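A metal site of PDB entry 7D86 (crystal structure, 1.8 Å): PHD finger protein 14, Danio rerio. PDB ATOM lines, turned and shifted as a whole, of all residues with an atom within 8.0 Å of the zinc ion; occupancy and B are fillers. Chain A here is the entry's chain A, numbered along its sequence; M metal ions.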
ATOM      1  N   SER A  74      -7.897   4.781  22.633  1.00  0.00           N
ATOM      2  CA  SER A  74      -9.176   4.096  22.591  1.00  0.00           C
ATOM      3  C   SER A  74      -9.115   3.028  21.511  1.00  0.00           C
ATOM      4  O   SER A  74      -8.365   3.144  20.547  1.00  0.00           O
ATOM      5  CB  SER A  74     -10.326   5.068  22.299  1.00  0.00           C
ATOM      6  OG  SER A  74     -10.500   5.981  23.381  1.00  0.00           O
ATOM      7  N   CYS A  75      -9.909   1.970  21.685  1.00  0.00           N
ATOM      8  CA  CYS A  75      -9.966   0.910  20.694  1.00  0.00           C
ATOM      9  C   CYS A  75     -10.928   1.285  19.576  1.00  0.00           C
ATOM     10  O   CYS A  75     -11.995   1.844  19.827  1.00  0.00           O
ATOM     11  CB  CYS A  75     -10.402  -0.411  21.345  1.00  0.00           C
ATOM     12  SG  CYS A  75     -10.365  -1.829  20.228  1.00  0.00           S
ATOM     13  N   GLU A  76     -10.538   0.981  18.337  1.00  0.00           N
ATOM     14  CA  GLU A  76     -11.440   1.197  17.218  1.00  0.00           C
ATOM     15  C   GLU A  76     -12.647   0.265  17.256  1.00  0.00           C
ATOM     16  O   GLU A  76     -13.631   0.513  16.563  1.00  0.00           O
ATOM     17  CB  GLU A  76     -10.700   0.999  15.897  1.00  0.00           C
ATOM     18  CG  GLU A  76      -9.602   2.040  15.656  1.00  0.00           C
ATOM     19  CD  GLU A  76     -10.146   3.447  15.630  1.00  0.00           C
ATOM     20  OE1 GLU A  76     -11.109   3.712  14.872  1.00  0.00           O
ATOM     21  OE2 GLU A  76      -9.617   4.309  16.374  1.00  0.00           O
ATOM     22  N   LEU A  77     -12.592  -0.795  18.068  1.00  0.00           N
ATOM     23  CA  LEU A  77     -13.560  -1.883  17.960  1.00  0.00           C
ATOM     24  C   LEU A  77     -14.414  -2.063  19.203  1.00  0.00           C
ATOM     25  O   LEU A  77     -15.303  -2.918  19.193  1.00  0.00           O
ATOM     26  CB  LEU A  77     -12.844  -3.206  17.658  1.00  0.00           C
ATOM     27  CG  LEU A  77     -11.897  -3.258  16.461  1.00  0.00           C
ATOM     28  CD1 LEU A  77     -11.186  -4.605  16.451  1.00  0.00           C
ATOM     29  CD2 LEU A  77     -12.653  -3.039  15.142  1.00  0.00           C
ATOM     30  N   CYS A  78     -14.171  -1.298  20.267  1.00  0.00           N
ATOM     31  CA  CYS A  78     -14.900  -1.473  21.518  1.00  0.00           C
ATOM     32  C   CYS A  78     -14.717  -0.218  22.369  1.00  0.00           C
ATOM     33  O   CYS A  78     -13.801   0.583  22.107  1.00  0.00           O
ATOM     34  CB  CYS A  78     -14.390  -2.714  22.276  1.00  0.00           C
ATOM     35  SG  CYS A  78     -12.905  -2.370  23.244  1.00  0.00           S
ATOM     36  N   PRO A  79     -15.560  -0.015  23.378  1.00  0.00           N
ATOM     37  CA  PRO A  79     -15.465   1.202  24.186  1.00  0.00           C
ATOM     38  C   PRO A  79     -14.504   1.128  25.370  1.00  0.00           C
ATOM     39  O   PRO A  79     -14.282   2.155  26.028  1.00  0.00           O
ATOM     40  CB  PRO A  79     -16.904   1.399  24.689  1.00  0.00           C
ATOM     41  CG  PRO A  79     -17.445   0.014  24.787  1.00  0.00           C
ATOM     42  CD  PRO A  79     -16.820  -0.749  23.626  1.00  0.00           C
ATOM     43  N   SER A  80     -13.928  -0.034  25.652  1.00  0.00           N
ATOM     44  CA  SER A  80     -13.044  -0.167  26.799  1.00  0.00           C
ATOM     45  C   SER A  80     -11.732   0.579  26.584  1.00  0.00           C
ATOM     46  O   SER A  80     -11.144   0.517  25.495  1.00  0.00           O
ATOM     47  CB  SER A  80     -12.747  -1.631  27.084  1.00  0.00           C
ATOM     48  OG  SER A  80     -11.726  -1.771  28.058  1.00  0.00           O
ATOM     49  N   GLN A  81     -11.267   1.277  27.612  1.00  0.00           N
ATOM     50  CA  GLN A  81      -9.941   1.879  27.578  1.00  0.00           C
ATOM     51  C   GLN A  81      -8.955   1.144  28.467  1.00  0.00           C
ATOM     52  O   GLN A  81      -7.809   1.573  28.599  1.00  0.00           O
ATOM     53  CB  GLN A  81     -10.021   3.359  27.965  1.00  0.00           C
ATOM     54  CG  GLN A  81     -10.744   4.177  26.911  1.00  0.00           C
ATOM     55  CD  GLN A  81     -10.903   5.633  27.286  1.00  0.00           C
ATOM     56  OE1 GLN A  81     -10.517   6.041  28.384  1.00  0.00           O
ATOM     57  NE2 GLN A  81     -11.464   6.425  26.386  1.00  0.00           N
ATOM     58  N   ASP A  82      -9.362   0.030  29.066  1.00  0.00           N
ATOM     59  CA  ASP A  82      -8.444  -0.828  29.793  1.00  0.00           C
ATOM     60  C   ASP A  82      -7.787  -1.829  28.850  1.00  0.00           C
ATOM     61  O   ASP A  82      -8.064  -1.861  27.636  1.00  0.00           O
ATOM     62  CB  ASP A  82      -9.174  -1.527  30.932  1.00  0.00           C
ATOM     63  CG  ASP A  82      -9.816  -0.552  31.903  1.00  0.00           C
ATOM     64  OD1 ASP A  82      -9.180   0.480  32.209  1.00  0.00           O
ATOM     65  OD2 ASP A  82     -10.950  -0.805  32.342  1.00  0.00           O
ATOM     66  N   ILE A  84      -4.604  -4.001  26.887  1.00  0.00           N
ATOM     67  CA  ILE A  84      -3.376  -3.699  26.172  1.00  0.00           C
ATOM     68  C   ILE A  84      -3.687  -3.580  24.682  1.00  0.00           C
ATOM     69  O   ILE A  84      -4.579  -4.263  24.156  1.00  0.00           O
ATOM     70  CB  ILE A  84      -2.286  -4.754  26.479  1.00  0.00           C
ATOM     71  CG1 ILE A  84      -0.896  -4.140  26.291  1.00  0.00           C
ATOM     72  CG2 ILE A  84      -2.438  -6.002  25.630  1.00  0.00           C
ATOM     73  CD1 ILE A  84       0.220  -5.008  26.829  1.00  0.00           C
ATOM     74  N   PHE A  85      -2.967  -2.676  24.018  1.00  0.00           N
ATOM     75  CA  PHE A  85      -3.279  -2.229  22.672  1.00  0.00           C
ATOM     76  C   PHE A  85      -2.112  -2.478  21.724  1.00  0.00           C
ATOM     77  O   PHE A  85      -0.948  -2.534  22.125  1.00  0.00           O
ATOM     78  CB  PHE A  85      -3.602  -0.734  22.629  1.00  0.00           C
ATOM     79  CG  PHE A  85      -4.852  -0.354  23.357  1.00  0.00           C
ATOM     80  CD1 PHE A  85      -4.859  -0.204  24.732  1.00  0.00           C
ATOM     81  CD2 PHE A  85      -6.030  -0.120  22.642  1.00  0.00           C
ATOM     82  CE1 PHE A  85      -6.012   0.165  25.396  1.00  0.00           C
ATOM     83  CE2 PHE A  85      -7.182   0.249  23.306  1.00  0.00           C
ATOM     84  CZ  PHE A  85      -7.180   0.387  24.691  1.00  0.00           C
ATOM     85  N   TRP A  93      -5.596   2.407  17.058  1.00  0.00           N
ATOM     86  CA  TRP A  93      -5.278   1.440  18.092  1.00  0.00           C
ATOM     87  C   TRP A  93      -6.442   0.475  18.287  1.00  0.00           C
ATOM     88  O   TRP A  93      -7.617   0.863  18.176  1.00  0.00           O
ATOM     89  CB  TRP A  93      -4.952   2.147  19.417  1.00  0.00           C
ATOM     90  CG  TRP A  93      -3.725   3.006  19.288  1.00  0.00           C
ATOM     91  CD1 TRP A  93      -3.668   4.304  18.868  1.00  0.00           C
ATOM     92  CD2 TRP A  93      -2.384   2.612  19.562  1.00  0.00           C
ATOM     93  NE1 TRP A  93      -2.362   4.747  18.876  1.00  0.00           N
ATOM     94  CE2 TRP A  93      -1.551   3.720  19.298  1.00  0.00           C
ATOM     95  CE3 TRP A  93      -1.793   1.427  20.019  1.00  0.00           C
ATOM     96  CZ2 TRP A  93      -0.169   3.682  19.471  1.00  0.00           C
ATOM     97  CZ3 TRP A  93      -0.429   1.387  20.186  1.00  0.00           C
ATOM     98  CH2 TRP A  93       0.373   2.501  19.914  1.00  0.00           C
ATOM     99  N   VAL A  94      -6.105  -0.777  18.547  1.00  0.00           N
ATOM    100  CA  VAL A  94      -7.095  -1.798  18.898  1.00  0.00           C
ATOM    101  C   VAL A  94      -6.536  -2.657  20.030  1.00  0.00           C
ATOM    102  O   VAL A  94      -5.318  -2.852  20.144  1.00  0.00           O
ATOM    103  CB  VAL A  94      -7.475  -2.684  17.686  1.00  0.00           C
ATOM    104  CG1 VAL A  94      -8.219  -1.872  16.635  1.00  0.00           C
ATOM    105  CG2 VAL A  94      -6.229  -3.320  17.077  1.00  0.00           C
ATOM    106  N   HIS A  95      -7.425  -3.200  20.855  1.00  0.00           N
ATOM    107  CA  HIS A  95      -7.015  -4.210  21.822  1.00  0.00           C
ATOM    108  C   HIS A  95      -6.441  -5.428  21.113  1.00  0.00           C
ATOM    109  O   HIS A  95      -6.934  -5.851  20.053  1.00  0.00           O
ATOM    110  CB  HIS A  95      -8.198  -4.675  22.699  1.00  0.00           C
ATOM    111  CG  HIS A  95      -8.698  -3.637  23.640  1.00  0.00           C
ATOM    112  ND1 HIS A  95      -9.911  -3.014  23.477  1.00  0.00           N
ATOM    113  CD2 HIS A  95      -8.150  -3.113  24.758  1.00  0.00           C
ATOM    114  CE1 HIS A  95     -10.092  -2.138  24.441  1.00  0.00           C
ATOM    115  NE2 HIS A  95      -9.030  -2.180  25.243  1.00  0.00           N
ATOM    116  N   VAL A  96      -5.394  -6.015  21.699  1.00  0.00           N
ATOM    117  CA  VAL A  96      -4.958  -7.331  21.255  1.00  0.00           C
ATOM    118  C   VAL A  96      -6.128  -8.308  21.320  1.00  0.00           C
ATOM    119  O   VAL A  96      -6.350  -9.101  20.386  1.00  0.00           O
ATOM    120  CB  VAL A  96      -3.769  -7.824  22.104  1.00  0.00           C
ATOM    121  CG1 VAL A  96      -3.531  -9.299  21.870  1.00  0.00           C
ATOM    122  CG2 VAL A  96      -2.515  -7.003  21.788  1.00  0.00           C
ATOM    123  N   VAL A  97      -6.912  -8.264  22.395  1.00  0.00           N
ATOM    124  CA  VAL A  97      -8.000  -9.245  22.530  1.00  0.00           C
ATOM    125  C   VAL A  97      -9.066  -9.000  21.472  1.00  0.00           C
ATOM    126  O   VAL A  97      -9.614  -9.955  20.898  1.00  0.00           O
ATOM    127  CB  VAL A  97      -8.559  -9.217  23.962  1.00  0.00           C
ATOM    128  CG1 VAL A  97      -9.410  -7.984  24.219  1.00  0.00           C
ATOM    129  CG2 VAL A  97      -9.355 -10.479  24.231  1.00  0.00           C
ATOM    130  N   CYS A  98      -9.359  -7.748  21.147  1.00  0.00           N
ATOM    131  CA  CYS A  98     -10.354  -7.502  20.101  1.00  0.00           C
ATOM    132  C   CYS A  98      -9.860  -8.016  18.753  1.00  0.00           C
ATOM    133  O   CYS A  98     -10.647  -8.536  17.944  1.00  0.00           O
ATOM    134  CB  CYS A  98     -10.698  -6.011  20.026  1.00  0.00           C
ATOM    135  SG  CYS A  98     -11.707  -5.424  21.421  1.00  0.00           S
ATOM    136  N   ALA A  99      -8.548  -7.922  18.519  1.00  0.00           N
ATOM    137  CA  ALA A  99      -8.002  -8.422  17.261  1.00  0.00           C
ATOM    138  C   ALA A  99      -8.111  -9.950  17.178  1.00  0.00           C
ATOM    139  O   ALA A  99      -8.249 -10.487  16.083  1.00  0.00           O
ATOM    140  CB  ALA A  99      -6.542  -7.988  17.112  1.00  0.00           C
ATOM    141  N   VAL A 102     -12.513 -10.537  16.708  1.00  0.00           N
ATOM    142  CA  VAL A 102     -13.311  -9.957  15.635  1.00  0.00           C
ATOM    143  C   VAL A 102     -12.970 -10.669  14.327  1.00  0.00           C
ATOM    144  O   VAL A 102     -11.798 -10.725  13.932  1.00  0.00           O
ATOM    145  CB  VAL A 102     -13.090  -8.435  15.526  1.00  0.00           C
ATOM    146  CG1 VAL A 102     -13.831  -7.878  14.304  1.00  0.00           C
ATOM    147  CG2 VAL A 102     -13.579  -7.735  16.805  1.00  0.00           C
ATOM    148  N   GLY A 143     -18.161   0.538  17.877  1.00  0.00           N
ATOM    149  CA  GLY A 143     -17.235  -0.507  17.563  1.00  0.00           C
ATOM    150  C   GLY A 143     -17.912  -1.692  16.911  1.00  0.00           C
ATOM    151  O   GLY A 143     -18.945  -1.570  16.242  1.00  0.00           O
ATOM    152  N   VAL A 144     -17.329  -2.859  17.115  1.00  0.00           N
ATOM    153  CA  VAL A 144     -17.735  -4.080  16.432  1.00  0.00           C
ATOM    154  C   VAL A 144     -18.047  -5.133  17.491  1.00  0.00           C
ATOM    155  O   VAL A 144     -17.244  -5.347  18.411  1.00  0.00           O
ATOM    156  CB  VAL A 144     -16.642  -4.575  15.462  1.00  0.00           C
ATOM    157  CG1 VAL A 144     -17.029  -5.913  14.850  1.00  0.00           C
ATOM    158  CG2 VAL A 144     -16.427  -3.561  14.357  1.00  0.00           C
ATOM    159  N   HIS A 158     -19.420  -6.701  22.674  1.00  0.00           N
ATOM    160  CA  HIS A 158     -18.032  -6.334  22.418  1.00  0.00           C
ATOM    161  C   HIS A 158     -17.115  -7.415  22.975  1.00  0.00           C
ATOM    162  O   HIS A 158     -17.440  -8.090  23.959  1.00  0.00           O
ATOM    163  CB  HIS A 158     -17.675  -5.000  23.086  1.00  0.00           C
ATOM    164  CG  HIS A 158     -18.439  -3.839  22.553  1.00  0.00           C
ATOM    165  ND1 HIS A 158     -19.342  -3.122  23.314  1.00  0.00           N
ATOM    166  CD2 HIS A 158     -18.435  -3.254  21.330  1.00  0.00           C
ATOM    167  CE1 HIS A 158     -19.854  -2.150  22.581  1.00  0.00           C
ATOM    168  NE2 HIS A 158     -19.318  -2.216  21.373  1.00  0.00           N
ATOM    169  N   VAL A 159     -15.929  -7.555  22.358  1.00  0.00           N
ATOM    170  CA  VAL A 159     -14.982  -8.562  22.810  1.00  0.00           C
ATOM    171  C   VAL A 159     -14.577  -8.310  24.255  1.00  0.00           C
ATOM    172  O   VAL A 159     -14.491  -9.241  25.062  1.00  0.00           O
ATOM    173  CB  VAL A 159     -13.751  -8.600  21.889  1.00  0.00           C
ATOM    174  CG1 VAL A 159     -12.721  -9.586  22.430  1.00  0.00           C
ATOM    175  CG2 VAL A 159     -14.167  -8.962  20.473  1.00  0.00           C
ATOM    176  N   THR A 160     -14.325  -7.046  24.614  1.00  0.00           N
ATOM    177  CA  THR A 160     -13.870  -6.740  25.963  1.00  0.00           C
ATOM    178  C   THR A 160     -15.005  -6.819  26.978  1.00  0.00           C
ATOM    179  O   THR A 160     -14.765  -7.107  28.152  1.00  0.00           O
ATOM    180  CB  THR A 160     -13.221  -5.358  26.011  1.00  0.00           C
ATOM    181  OG1 THR A 160     -14.052  -4.402  25.339  1.00  0.00           O
ATOM    182  CG2 THR A 160     -11.859  -5.401  25.321  1.00  0.00           C
ATOM    183  N   CYS A 161     -16.247  -6.546  26.552  1.00  0.00           N
ATOM    184  CA  CYS A 161     -17.382  -6.751  27.426  1.00  0.00           C
ATOM    185  C   CYS A 161     -17.579  -8.235  27.726  1.00  0.00           C
ATOM    186  O   CYS A 161     -17.822  -8.622  28.875  1.00  0.00           O
ATOM    187  CB  CYS A 161     -18.642  -6.146  26.803  1.00  0.00           C
ATOM    188  SG  CYS A 161     -18.648  -4.309  26.728  1.00  0.00           S
HETATM  189 ZN    ZN M   1     -11.221  -3.203  21.974  1.00  0.00          ZN
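The side-chain sulfur (SG) of Cys 75 sits close to the backbone NH (N) of Leu 77, 3.3 Å away. NE2 of His 95 sits at hydrogen-bond distance from O of Asp 82 (2.6 Å). The side-chain sulfur (SG) of Cys 78 lies close to the backbone NH (N) of Ser 80 (3.5 Å). NE2 of His 95 lies close to O of Ser 80 (3.4 Å). SG of Cys 78 sits close to OG1 of Thr 160, at 3.1 Å.
The zinc ion is bound by a ring nitrogen (ND1) of His 95 (2.0 Å), the side-chain sulfur of Cys 78 (2.3 Å), the side-chain sulfur of Cys 98 (2.3 Å) and the side-chain sulfur of Cys 75 (2.4 Å).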
